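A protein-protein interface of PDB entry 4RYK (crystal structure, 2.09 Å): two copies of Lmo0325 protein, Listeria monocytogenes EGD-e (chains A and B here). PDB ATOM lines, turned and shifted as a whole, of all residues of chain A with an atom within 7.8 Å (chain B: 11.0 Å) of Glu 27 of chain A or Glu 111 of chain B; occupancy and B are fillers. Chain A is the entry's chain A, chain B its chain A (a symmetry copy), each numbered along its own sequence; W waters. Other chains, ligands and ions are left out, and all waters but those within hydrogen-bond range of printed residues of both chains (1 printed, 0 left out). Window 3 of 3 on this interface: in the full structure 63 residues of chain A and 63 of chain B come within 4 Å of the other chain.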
ATOM      1  N   ARG A  18      -7.369  29.652  14.067  1.00  0.00           N
ATOM      2  CA  ARG A  18      -6.017  29.868  14.547  1.00  0.00           C
ATOM      3  C   ARG A  18      -5.681  31.349  14.657  1.00  0.00           C
ATOM      4  O   ARG A  18      -5.212  31.812  15.714  1.00  0.00           O
ATOM      5  CB  ARG A  18      -5.002  29.151  13.636  1.00  0.00           C
ATOM      6  CG  ARG A  18      -3.585  29.454  13.994  1.00  0.00           C
ATOM      7  CD  ARG A  18      -2.595  28.757  13.094  1.00  0.00           C
ATOM      8  NE  ARG A  18      -2.532  29.291  11.747  1.00  0.00           N
ATOM      9  CZ  ARG A  18      -1.988  30.453  11.393  1.00  0.00           C
ATOM     10  NH1 ARG A  18      -1.499  31.290  12.302  1.00  0.00           N
ATOM     11  NH2 ARG A  18      -1.967  30.789  10.108  1.00  0.00           N
ATOM     12  N   LYS A  21      -7.340  33.299  17.446  1.00  0.00           N
ATOM     13  CA  LYS A  21      -6.783  33.015  18.781  1.00  0.00           C
ATOM     14  C   LYS A  21      -5.377  33.547  18.995  1.00  0.00           C
ATOM     15  O   LYS A  21      -4.821  33.414  20.096  1.00  0.00           O
ATOM     16  CB  LYS A  21      -6.815  31.496  19.045  1.00  0.00           C
ATOM     17  CG  LYS A  21      -8.250  30.951  19.127  1.00  0.00           C
ATOM     18  CD  LYS A  21      -8.245  29.530  19.630  1.00  0.00           C
ATOM     19  CE  LYS A  21      -9.596  28.841  19.546  1.00  0.00           C
ATOM     20  NZ  LYS A  21     -10.704  29.663  20.091  1.00  0.00           N
ATOM     21  N   GLY A  22      -4.823  34.179  17.967  1.00  0.00           N
ATOM     22  CA  GLY A  22      -3.486  34.710  18.014  1.00  0.00           C
ATOM     23  C   GLY A  22      -2.422  33.618  18.045  1.00  0.00           C
ATOM     24  O   GLY A  22      -1.358  33.850  18.589  1.00  0.00           O
ATOM     25  N   LEU A  23      -2.714  32.446  17.478  1.00  0.00           N
ATOM     26  CA  LEU A  23      -1.766  31.327  17.467  1.00  0.00           C
ATOM     27  C   LEU A  23      -0.929  31.296  16.213  1.00  0.00           C
ATOM     28  O   LEU A  23      -1.398  31.645  15.110  1.00  0.00           O
ATOM     29  CB  LEU A  23      -2.499  29.994  17.609  1.00  0.00           C
ATOM     30  CG  LEU A  23      -3.288  29.854  18.928  1.00  0.00           C
ATOM     31  CD1 LEU A  23      -4.272  28.708  18.851  1.00  0.00           C
ATOM     32  CD2 LEU A  23      -2.384  29.702  20.133  1.00  0.00           C
ATOM     33  N   THR A  24       0.325  30.884  16.374  1.00  0.00           N
ATOM     34  CA  THR A  24       1.232  30.810  15.228  1.00  0.00           C
ATOM     35  C   THR A  24       1.066  29.438  14.554  1.00  0.00           C
ATOM     36  O   THR A  24       0.519  28.512  15.158  1.00  0.00           O
ATOM     37  CB  THR A  24       2.700  31.000  15.633  1.00  0.00           C
ATOM     38  OG1 THR A  24       3.068  29.992  16.571  1.00  0.00           O
ATOM     39  CG2 THR A  24       2.917  32.344  16.289  1.00  0.00           C
ATOM     40  N   GLN A  25       1.501  29.347  13.300  1.00  0.00           N
ATOM     41  CA  GLN A  25       1.597  28.087  12.598  1.00  0.00           C
ATOM     42  C   GLN A  25       2.568  27.200  13.283  1.00  0.00           C
ATOM     43  O   GLN A  25       2.353  26.021  13.406  1.00  0.00           O
ATOM     44  CB  GLN A  25       2.066  28.318  11.165  1.00  0.00           C
ATOM     45  CG  GLN A  25       1.014  28.995  10.291  1.00  0.00           C
ATOM     46  CD  GLN A  25       1.451  29.110   8.853  1.00  0.00           C
ATOM     47  OE1 GLN A  25       2.538  29.560   8.584  1.00  0.00           O
ATOM     48  NE2 GLN A  25       0.592  28.728   7.930  1.00  0.00           N
ATOM     49  N   LYS A  26       3.671  27.771  13.719  1.00  0.00           N
ATOM     50  CA  LYS A  26       4.635  27.009  14.458  1.00  0.00           C
ATOM     51  C   LYS A  26       4.018  26.301  15.668  1.00  0.00           C
ATOM     52  O   LYS A  26       4.268  25.118  15.896  1.00  0.00           O
ATOM     53  CB  LYS A  26       5.787  27.884  14.911  1.00  0.00           C
ATOM     54  CG  LYS A  26       6.915  27.058  15.490  1.00  0.00           C
ATOM     55  CD  LYS A  26       7.878  27.921  16.281  1.00  0.00           C
ATOM     56  CE  LYS A  26       9.022  27.090  16.835  1.00  0.00           C
ATOM     57  NZ  LYS A  26      10.238  27.943  16.828  1.00  0.00           N
ATOM     58  N   GLU A  27       3.239  26.979  16.473  1.00  0.00           N
ATOM     59  CA  GLU A  27       2.732  26.266  17.629  1.00  0.00           C
ATOM     60  C   GLU A  27       1.546  25.360  17.339  1.00  0.00           C
ATOM     61  O   GLU A  27       1.302  24.415  18.069  1.00  0.00           O
ATOM     62  CB  GLU A  27       2.468  27.223  18.778  1.00  0.00           C
ATOM     63  CG  GLU A  27       1.189  27.988  18.748  1.00  0.00           C
ATOM     64  CD  GLU A  27       1.290  29.221  19.660  1.00  0.00           C
ATOM     65  OE1 GLU A  27       1.330  29.063  20.912  1.00  0.00           O
ATOM     66  OE2 GLU A  27       1.331  30.345  19.123  1.00  0.00           O
ATOM     67  N   VAL A  28       0.826  25.595  16.257  1.00  0.00           N
ATOM     68  CA  VAL A  28      -0.282  24.715  15.958  1.00  0.00           C
ATOM     69  C   VAL A  28       0.203  23.400  15.299  1.00  0.00           C
ATOM     70  O   VAL A  28      -0.288  22.330  15.621  1.00  0.00           O
ATOM     71  CB  VAL A  28      -1.323  25.409  15.087  1.00  0.00           C
ATOM     72  CG1 VAL A  28      -2.258  24.403  14.478  1.00  0.00           C
ATOM     73  CG2 VAL A  28      -2.113  26.405  15.907  1.00  0.00           C
ATOM     74  N   TYR A  29       1.175  23.487  14.395  1.00  0.00           N
ATOM     75  CA  TYR A  29       1.499  22.369  13.519  1.00  0.00           C
ATOM     76  C   TYR A  29       2.751  21.557  13.850  1.00  0.00           C
ATOM     77  O   TYR A  29       2.865  20.418  13.370  1.00  0.00           O
ATOM     78  CB  TYR A  29       1.563  22.842  12.068  1.00  0.00           C
ATOM     79  CG  TYR A  29       0.230  23.361  11.569  1.00  0.00           C
ATOM     80  CD1 TYR A  29      -0.832  22.491  11.319  1.00  0.00           C
ATOM     81  CD2 TYR A  29       0.014  24.712  11.412  1.00  0.00           C
ATOM     82  CE1 TYR A  29      -2.037  22.956  10.865  1.00  0.00           C
ATOM     83  CE2 TYR A  29      -1.190  25.196  10.957  1.00  0.00           C
ATOM     84  CZ  TYR A  29      -2.219  24.315  10.695  1.00  0.00           C
ATOM     85  OH  TYR A  29      -3.411  24.830  10.266  1.00  0.00           O
ATOM     86  N   THR A  30       3.638  22.115  14.676  1.00  0.00           N
ATOM     87  CA  THR A  30       4.904  21.502  14.964  1.00  0.00           C
ATOM     88  C   THR A  30       4.713  20.142  15.597  1.00  0.00           C
ATOM     89  O   THR A  30       3.932  19.987  16.525  1.00  0.00           O
ATOM     90  CB  THR A  30       5.771  22.334  15.927  1.00  0.00           C
ATOM     91  OG1 THR A  30       6.000  23.604  15.350  1.00  0.00           O
ATOM     92  CG2 THR A  30       7.150  21.687  16.098  1.00  0.00           C
ATOM     93  N   GLY A  31       5.409  19.162  15.036  1.00  0.00           N
ATOM     94  CA  GLY A  31       5.304  17.773  15.449  1.00  0.00           C
ATOM     95  C   GLY A  31       4.093  17.080  14.842  1.00  0.00           C
ATOM     96  O   GLY A  31       3.914  15.883  15.026  1.00  0.00           O
ATOM     97  N   ILE A  32       3.251  17.791  14.095  1.00  0.00           N
ATOM     98  CA  ILE A  32       2.093  17.104  13.482  1.00  0.00           C
ATOM     99  C   ILE A  32       2.340  16.973  11.987  1.00  0.00           C
ATOM    100  O   ILE A  32       2.379  15.882  11.455  1.00  0.00           O
ATOM    101  CB  ILE A  32       0.770  17.857  13.769  1.00  0.00           C
ATOM    102  CG1 ILE A  32       0.470  17.863  15.274  1.00  0.00           C
ATOM    103  CG2 ILE A  32      -0.407  17.234  13.029  1.00  0.00           C
ATOM    104  CD1 ILE A  32      -0.559  18.884  15.680  1.00  0.00           C
ATOM    105  N   ARG A  35       6.027  22.406   7.925  1.00  0.00           N
ATOM    106  CA  ARG A  35       5.740  23.765   7.639  1.00  0.00           C
ATOM    107  C   ARG A  35       4.979  23.920   6.348  1.00  0.00           C
ATOM    108  O   ARG A  35       3.908  24.490   6.323  1.00  0.00           O
ATOM    109  CB  ARG A  35       7.054  24.557   7.591  1.00  0.00           C
ATOM    110  CG  ARG A  35       6.928  26.018   7.139  1.00  0.00           C
ATOM    111  CD  ARG A  35       6.338  26.969   8.195  1.00  0.00           C
ATOM    112  NE  ARG A  35       5.693  26.264   9.319  1.00  0.00           N
ATOM    113  CZ  ARG A  35       4.379  26.031   9.466  1.00  0.00           C
ATOM    114  NH1 ARG A  35       3.492  26.468   8.550  1.00  0.00           N
ATOM    115  NH2 ARG A  35       3.955  25.336  10.546  1.00  0.00           N
ATOM    116  N   GLU A  55      -5.340  15.897  15.909  1.00  0.00           N
ATOM    117  CA  GLU A  55      -4.221  16.496  16.663  1.00  0.00           C
ATOM    118  C   GLU A  55      -4.204  17.997  16.475  1.00  0.00           C
ATOM    119  O   GLU A  55      -3.923  18.752  17.415  1.00  0.00           O
ATOM    120  CB  GLU A  55      -2.892  15.888  16.233  1.00  0.00           C
ATOM    121  CG  GLU A  55      -2.794  14.397  16.538  1.00  0.00           C
ATOM    122  CD  GLU A  55      -1.584  13.750  15.907  1.00  0.00           C
ATOM    123  OE1 GLU A  55      -0.513  14.385  15.817  1.00  0.00           O
ATOM    124  OE2 GLU A  55      -1.697  12.572  15.508  1.00  0.00           O
ATOM    125  N   ILE A  56      -4.507  18.447  15.265  1.00  0.00           N
ATOM    126  CA  ILE A  56      -4.535  19.902  14.983  1.00  0.00           C
ATOM    127  C   ILE A  56      -5.652  20.560  15.771  1.00  0.00           C
ATOM    128  O   ILE A  56      -5.479  21.612  16.381  1.00  0.00           O
ATOM    129  CB  ILE A  56      -4.710  20.152  13.472  1.00  0.00           C
ATOM    130  CG1 ILE A  56      -3.410  19.760  12.761  1.00  0.00           C
ATOM    131  CG2 ILE A  56      -5.061  21.599  13.223  1.00  0.00           C
ATOM    132  CD1 ILE A  56      -3.566  19.473  11.275  1.00  0.00           C
ATOM    133  N   ARG A  59      -4.701  21.363  19.138  1.00  0.00           N
ATOM    134  CA  ARG A  59      -3.817  22.520  19.253  1.00  0.00           C
ATOM    135  C   ARG A  59      -4.549  23.870  19.209  1.00  0.00           C
ATOM    136  O   ARG A  59      -3.999  24.900  19.646  1.00  0.00           O
ATOM    137  CB  ARG A  59      -2.775  22.464  18.147  1.00  0.00           C
ATOM    138  CG  ARG A  59      -1.788  21.325  18.273  1.00  0.00           C
ATOM    139  CD  ARG A  59      -0.703  21.675  19.274  1.00  0.00           C
ATOM    140  NE  ARG A  59       0.221  20.579  19.368  1.00  0.00           N
ATOM    141  CZ  ARG A  59       1.258  20.406  18.575  1.00  0.00           C
ATOM    142  NH1 ARG A  59       1.542  21.257  17.608  1.00  0.00           N
ATOM    143  NH2 ARG A  59       2.027  19.355  18.756  1.00  0.00           N
ATOM    144  N   ILE A  60      -5.754  23.904  18.647  1.00  0.00           N
ATOM    145  CA  ILE A  60      -6.513  25.136  18.624  1.00  0.00           C
ATOM    146  C   ILE A  60      -7.657  25.055  19.614  1.00  0.00           C
ATOM    147  O   ILE A  60      -8.420  26.008  19.720  1.00  0.00           O
ATOM    148  CB  ILE A  60      -7.001  25.535  17.215  1.00  0.00           C
ATOM    149  CG1 ILE A  60      -7.869  24.442  16.576  1.00  0.00           C
ATOM    150  CG2 ILE A  60      -5.841  25.801  16.272  1.00  0.00           C
ATOM    151  CD1 ILE A  60      -8.791  24.950  15.499  1.00  0.00           C
ATOM    152  N   ILE B 105      -0.325  17.696  31.653  1.00  0.00           N
ATOM    153  CA  ILE B 105      -0.359  18.655  30.550  1.00  0.00           C
ATOM    154  C   ILE B 105       0.945  19.432  30.426  1.00  0.00           C
ATOM    155  O   ILE B 105       1.298  19.914  29.361  1.00  0.00           O
ATOM    156  CB  ILE B 105      -1.568  19.635  30.617  1.00  0.00           C
ATOM    157  CG1 ILE B 105      -1.422  20.657  31.713  1.00  0.00           C
ATOM    158  CG2 ILE B 105      -2.887  18.903  30.834  1.00  0.00           C
ATOM    159  CD1 ILE B 105      -2.670  21.483  31.855  1.00  0.00           C
ATOM    160  N   THR B 106       1.656  19.552  31.526  1.00  0.00           N
ATOM    161  CA  THR B 106       2.986  20.108  31.498  1.00  0.00           C
ATOM    162  C   THR B 106       3.960  19.279  30.646  1.00  0.00           C
ATOM    163  O   THR B 106       4.784  19.858  29.949  1.00  0.00           O
ATOM    164  CB  THR B 106       3.510  20.286  32.936  1.00  0.00           C
ATOM    165  OG1 THR B 106       3.025  21.533  33.440  1.00  0.00           O
ATOM    166  CG2 THR B 106       5.021  20.276  32.997  1.00  0.00           C
ATOM    167  N   LEU B 107       3.882  17.946  30.697  1.00  0.00           N
ATOM    168  CA  LEU B 107       4.824  17.104  29.925  1.00  0.00           C
ATOM    169  C   LEU B 107       4.629  17.183  28.401  1.00  0.00           C
ATOM    170  O   LEU B 107       5.583  17.069  27.642  1.00  0.00           O
ATOM    171  CB  LEU B 107       4.793  15.653  30.409  1.00  0.00           C
ATOM    172  CG  LEU B 107       5.191  15.542  31.875  1.00  0.00           C
ATOM    173  CD1 LEU B 107       5.185  14.073  32.271  1.00  0.00           C
ATOM    174  CD2 LEU B 107       6.540  16.218  32.166  1.00  0.00           C
ATOM    175  N   GLU B 108       3.406  17.402  27.950  1.00  0.00           N
ATOM    176  CA  GLU B 108       3.189  17.751  26.543  1.00  0.00           C
ATOM    177  C   GLU B 108       3.867  19.111  26.196  1.00  0.00           C
ATOM    178  O   GLU B 108       4.534  19.241  25.170  1.00  0.00           O
ATOM    179  CB  GLU B 108       1.682  17.771  26.231  1.00  0.00           C
ATOM    180  CG  GLU B 108       1.135  19.124  25.814  1.00  0.00           C
ATOM    181  CD  GLU B 108      -0.260  19.390  26.313  1.00  0.00           C
ATOM    182  OE1 GLU B 108      -1.052  18.429  26.395  1.00  0.00           O
ATOM    183  OE2 GLU B 108      -0.550  20.570  26.624  1.00  0.00           O
ATOM    184  N   ARG B 109       3.691  20.102  27.076  1.00  0.00           N
ATOM    185  CA  ARG B 109       4.133  21.508  26.883  1.00  0.00           C
ATOM    186  C   ARG B 109       4.068  22.096  25.471  1.00  0.00           C
ATOM    187  O   ARG B 109       5.006  22.701  24.974  1.00  0.00           O
ATOM    188  CB  ARG B 109       5.502  21.764  27.507  1.00  0.00           C
ATOM    189  CG  ARG B 109       5.461  22.672  28.738  1.00  0.00           C
ATOM    190  CD  ARG B 109       6.803  22.718  29.457  1.00  0.00           C
ATOM    191  NE  ARG B 109       7.285  21.374  29.805  1.00  0.00           N
ATOM    192  CZ  ARG B 109       8.001  20.566  29.008  1.00  0.00           C
ATOM    193  NH1 ARG B 109       8.354  20.930  27.767  1.00  0.00           N
ATOM    194  NH2 ARG B 109       8.360  19.366  29.461  1.00  0.00           N
ATOM    195  N   THR B 110       2.938  21.860  24.840  1.00  0.00           N
ATOM    196  CA  THR B 110       2.257  22.846  24.041  1.00  0.00           C
ATOM    197  C   THR B 110       2.408  24.236  24.698  1.00  0.00           C
ATOM    198  O   THR B 110       2.190  24.397  25.907  1.00  0.00           O
ATOM    199  CB  THR B 110       0.789  22.395  23.964  1.00  0.00           C
ATOM    200  OG1 THR B 110       0.752  21.173  23.230  1.00  0.00           O
ATOM    201  CG2 THR B 110      -0.103  23.375  23.290  1.00  0.00           C
ATOM    202  N   GLU B 111       2.807  25.221  23.893  1.00  0.00           N
ATOM    203  CA  GLU B 111       2.913  26.625  24.333  1.00  0.00           C
ATOM    204  C   GLU B 111       1.564  27.234  24.767  1.00  0.00           C
ATOM    205  O   GLU B 111       1.501  27.942  25.756  1.00  0.00           O
ATOM    206  CB  GLU B 111       3.520  27.494  23.213  1.00  0.00           C
ATOM    207  CG  GLU B 111       4.935  27.102  22.806  1.00  0.00           C
ATOM    208  CD  GLU B 111       5.901  27.159  23.976  1.00  0.00           C
ATOM    209  OE1 GLU B 111       6.538  26.130  24.307  1.00  0.00           O
ATOM    210  OE2 GLU B 111       6.002  28.240  24.589  1.00  0.00           O
ATOM    211  N   GLN B 112       0.492  26.954  24.026  1.00  0.00           N
ATOM    212  CA  GLN B 112      -0.852  27.508  24.298  1.00  0.00           C
ATOM    213  C   GLN B 112      -1.601  26.800  25.450  1.00  0.00           C
ATOM    214  O   GLN B 112      -2.704  27.221  25.833  1.00  0.00           O
ATOM    215  CB  GLN B 112      -1.725  27.477  23.025  1.00  0.00           C
ATOM    216  CG  GLN B 112      -1.981  26.089  22.403  1.00  0.00           C
ATOM    217  CD  GLN B 112      -0.940  25.692  21.344  1.00  0.00           C
ATOM    218  OE1 GLN B 112       0.268  25.834  21.562  1.00  0.00           O
ATOM    219  NE2 GLN B 112      -1.401  25.181  20.206  1.00  0.00           N
ATOM    220  N   SER B 113      -1.013  25.738  26.003  1.00  0.00           N
ATOM    221  CA  SER B 113      -1.565  25.139  27.187  1.00  0.00           C
ATOM    222  C   SER B 113      -1.293  26.088  28.374  1.00  0.00           C
ATOM    223  O   SER B 113      -1.750  25.819  29.495  1.00  0.00           O
ATOM    224  CB  SER B 113      -0.993  23.734  27.375  1.00  0.00           C
ATOM    225  OG  SER B 113       0.423  23.729  27.349  1.00  0.00           O
ATOM    226  N   GLU B 114      -0.606  27.226  28.115  1.00  0.00           N
ATOM    227  CA  GLU B 114      -0.322  28.235  29.154  1.00  0.00           C
ATOM    228  C   GLU B 114      -1.572  28.684  29.894  1.00  0.00           C
ATOM    229  O   GLU B 114      -1.580  28.789  31.138  1.00  0.00           O
ATOM    230  CB  GLU B 114       0.377  29.483  28.599  1.00  0.00           C
ATOM    231  CG  GLU B 114       1.886  29.403  28.405  1.00  0.00           C
ATOM    232  CD  GLU B 114       2.651  28.934  29.634  1.00  0.00           C
ATOM    233  OE1 GLU B 114       3.287  27.853  29.533  1.00  0.00           O
ATOM    234  OE2 GLU B 114       2.623  29.632  30.687  1.00  0.00           O
ATOM    235  N   VAL B 115      -2.644  28.935  29.168  1.00  0.00           N
ATOM    236  CA  VAL B 115      -3.865  29.429  29.824  1.00  0.00           C
ATOM    237  C   VAL B 115      -4.489  28.342  30.645  1.00  0.00           C
ATOM    238  O   VAL B 115      -4.897  28.578  31.755  1.00  0.00           O
ATOM    239  CB  VAL B 115      -4.890  29.942  28.836  1.00  0.00           C
ATOM    240  CG1 VAL B 115      -6.087  30.526  29.551  1.00  0.00           C
ATOM    241  CG2 VAL B 115      -4.252  31.024  28.074  1.00  0.00           C
ATOM    242  N   ARG B 116      -4.538  27.132  30.116  1.00  0.00           N
ATOM    243  CA  ARG B 116      -5.113  26.027  30.892  1.00  0.00           C
ATOM    244  C   ARG B 116      -4.296  25.764  32.114  1.00  0.00           C
ATOM    245  O   ARG B 116      -4.846  25.540  33.205  1.00  0.00           O
ATOM    246  CB  ARG B 116      -5.246  24.784  30.034  1.00  0.00           C
ATOM    247  CG  ARG B 116      -6.383  24.925  29.039  1.00  0.00           C
ATOM    248  CD  ARG B 116      -6.532  23.675  28.194  1.00  0.00           C
ATOM    249  NE  ARG B 116      -7.686  23.677  27.278  1.00  0.00           N
ATOM    250  CZ  ARG B 116      -8.067  22.584  26.623  1.00  0.00           C
ATOM    251  NH1 ARG B 116      -7.393  21.449  26.787  1.00  0.00           N
ATOM    252  NH2 ARG B 116      -9.091  22.613  25.785  1.00  0.00           N
ATOM    253  N   LYS B 117      -2.985  25.808  31.967  1.00  0.00           N
ATOM    254  CA  LYS B 117      -2.102  25.647  33.146  1.00  0.00           C
ATOM    255  C   LYS B 117      -2.298  26.741  34.157  1.00  0.00           C
ATOM    256  O   LYS B 117      -2.318  26.477  35.354  1.00  0.00           O
ATOM    257  CB  LYS B 117      -0.651  25.594  32.741  1.00  0.00           C
ATOM    258  CG  LYS B 117      -0.348  24.317  31.988  1.00  0.00           C
ATOM    259  CD  LYS B 117       1.138  24.098  31.787  1.00  0.00           C
ATOM    260  CE  LYS B 117       1.717  24.968  30.702  1.00  0.00           C
ATOM    261  NZ  LYS B 117       2.706  24.158  29.924  1.00  0.00           N
ATOM    262  N   ALA B 118      -2.488  27.969  33.681  1.00  0.00           N
ATOM    263  CA  ALA B 118      -2.705  29.082  34.614  1.00  0.00           C
ATOM    264  C   ALA B 118      -3.995  28.859  35.391  1.00  0.00           C
ATOM    265  O   ALA B 118      -4.091  29.117  36.586  1.00  0.00           O
ATOM    266  CB  ALA B 118      -2.712  30.417  33.869  1.00  0.00           C
ATOM    267  N   ILE B 148      -1.845  36.045  32.660  1.00  0.00           N
ATOM    268  CA  ILE B 148      -1.828  35.126  31.522  1.00  0.00           C
ATOM    269  C   ILE B 148      -3.242  34.930  30.953  1.00  0.00           C
ATOM    270  O   ILE B 148      -3.451  34.909  29.760  1.00  0.00           O
ATOM    271  CB  ILE B 148      -1.204  33.784  31.918  1.00  0.00           C
ATOM    272  CG1 ILE B 148       0.315  33.917  31.942  1.00  0.00           C
ATOM    273  CG2 ILE B 148      -1.589  32.676  30.936  1.00  0.00           C
ATOM    274  CD1 ILE B 148       0.998  32.767  32.671  1.00  0.00           C
ATOM    275  N   ILE B 149      -4.206  34.788  31.827  1.00  0.00           N
ATOM    276  CA  ILE B 149      -5.569  34.527  31.411  1.00  0.00           C
ATOM    277  C   ILE B 149      -6.146  35.787  30.763  1.00  0.00           C
ATOM    278  O   ILE B 149      -6.704  35.743  29.686  1.00  0.00           O
ATOM    279  CB  ILE B 149      -6.420  34.109  32.623  1.00  0.00           C
ATOM    280  CG1 ILE B 149      -5.933  32.760  33.131  1.00  0.00           C
ATOM    281  CG2 ILE B 149      -7.907  34.074  32.243  1.00  0.00           C
ATOM    282  CD1 ILE B 149      -6.315  32.499  34.578  1.00  0.00           C
ATOM    283  N   TYR B 152      -4.546  36.309  27.279  1.00  0.00           N
ATOM    284  CA  TYR B 152      -5.042  35.392  26.258  1.00  0.00           C
ATOM    285  C   TYR B 152      -6.356  35.903  25.629  1.00  0.00           C
ATOM    286  O   TYR B 152      -6.523  35.915  24.425  1.00  0.00           O
ATOM    287  CB  TYR B 152      -5.298  33.998  26.868  1.00  0.00           C
ATOM    288  CG  TYR B 152      -5.952  33.060  25.870  1.00  0.00           C
ATOM    289  CD1 TYR B 152      -5.211  32.512  24.823  1.00  0.00           C
ATOM    290  CD2 TYR B 152      -7.299  32.760  25.935  1.00  0.00           C
ATOM    291  CE1 TYR B 152      -5.789  31.701  23.857  1.00  0.00           C
ATOM    292  CE2 TYR B 152      -7.896  31.901  25.005  1.00  0.00           C
ATOM    293  CZ  TYR B 152      -7.142  31.362  23.967  1.00  0.00           C
ATOM    294  OH  TYR B 152      -7.711  30.539  22.977  1.00  0.00           O
ATOM    295  N   GLU B 162     -14.075  27.292  23.929  1.00  0.00           N
ATOM    296  CA  GLU B 162     -12.915  27.320  24.819  1.00  0.00           C
ATOM    297  C   GLU B 162     -12.839  28.647  25.604  1.00  0.00           C
ATOM    298  O   GLU B 162     -12.603  28.658  26.797  1.00  0.00           O
ATOM    299  CB  GLU B 162     -11.636  27.086  23.999  1.00  0.00           C
ATOM    300  CG  GLU B 162     -10.339  27.198  24.802  1.00  0.00           C
ATOM    301  CD  GLU B 162     -10.130  25.992  25.697  1.00  0.00           C
ATOM    302  OE1 GLU B 162     -10.862  24.975  25.554  1.00  0.00           O
ATOM    303  OE2 GLU B 162      -9.221  26.012  26.515  1.00  0.00           O
HETATM  304  O   HOH W   1      -5.013  34.894  22.301  1.00  0.00           O
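Hydrophobic or aromatic side chains of chain B that line the printed part of chain A: Tyr 152.
Hydrophobic or aromatic side chains of chain A that line the printed part of chain B: Leu 23.
Along chain A the printed residues that touch a printed residue of chain B span positions 21 to 59.
Among the printed residues, 6 pairs touch across the chains.
Among the printed residues, no Asp or Glu carboxylate lies within 4 Å of a Lys or Arg side-chain nitrogen of the other chain.
Of the printed residues of chain B, Lys 21 of chain A touches Tyr 152.
Leu 23 of chain A touches just one residue of chain B: Gln 112.
No residue of chain B comes within 4 Å of Thr 24 of chain A.
No residue of chain B comes within 4 Å of Val 28 of chain A.
No residue of chain B comes within 4 Å of Thr 30 of chain A.
Printed residues of chain A within 4 Å of Glu 111 of chain B: Glu 27 (3.5 Å).
Of the printed residues of chain A, Gln 112 of chain B touches Leu 23, Glu 27 and Arg 59.
Of the printed residues of chain A, Tyr 152 of chain B touches Lys 21 (3.5 Å).
The nearest residue of chain B that does not touch Glu 27 of chain A is Thr 110 of chain B (5.5 Å).
The nearest printed residue of chain B that does not touch Lys 21 of chain A is Glu 162 of chain B (4.8 Å).
The backbone carbonyl oxygen (O) of Leu 23 of chain A lies within hydrogen-bond range of the guanidinium group (NH1) of Arg 18 of chain A (2.8 Å).
N of Thr 24 of chain A sits at hydrogen-bond distance from OE2 of Glu 27 of chain A, at 3.0 Å.
O of Glu 27 of chain A is in hydrogen-bond range of NH1 of Arg 59 of chain A (3.2 Å).
The guanidinium group of Arg 59 of chain A sits at hydrogen-bond distance from the backbone carbonyl oxygen of Val 28 of chain A.
The guanidinium group (NH1) of Arg 59 of chain A is in hydrogen-bond range of the backbone carbonyl oxygen (O) of Thr 30 of chain A (2.9 Å).
Water W1 bridges O of Lys 21 of chain A (2.7 Å) and O of Tyr 152 of chain B (2.8 Å).
No position is printed for both chains.
Tyr 152 of chain B touches Lys 21 of chain A (OH to CD, 3.5 Å).
CB of Gln 112 of chain B touches CD2 of Leu 23 of chain A (3.7 Å).
Glu 27 of chain A touches Glu 111 of chain B (OE1 to CB, 3.5 Å).
Thr 110 of chain B touches Arg 59 of chain A.
OE1 of Glu 27 of chain A lies close to OE1 of Gln 112 of chain B, 3.5 Å away.
O of Arg 59 of chain A sits at hydrogen-bond distance from NE2 of Gln 112 of chain B, 2.7 Å away.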
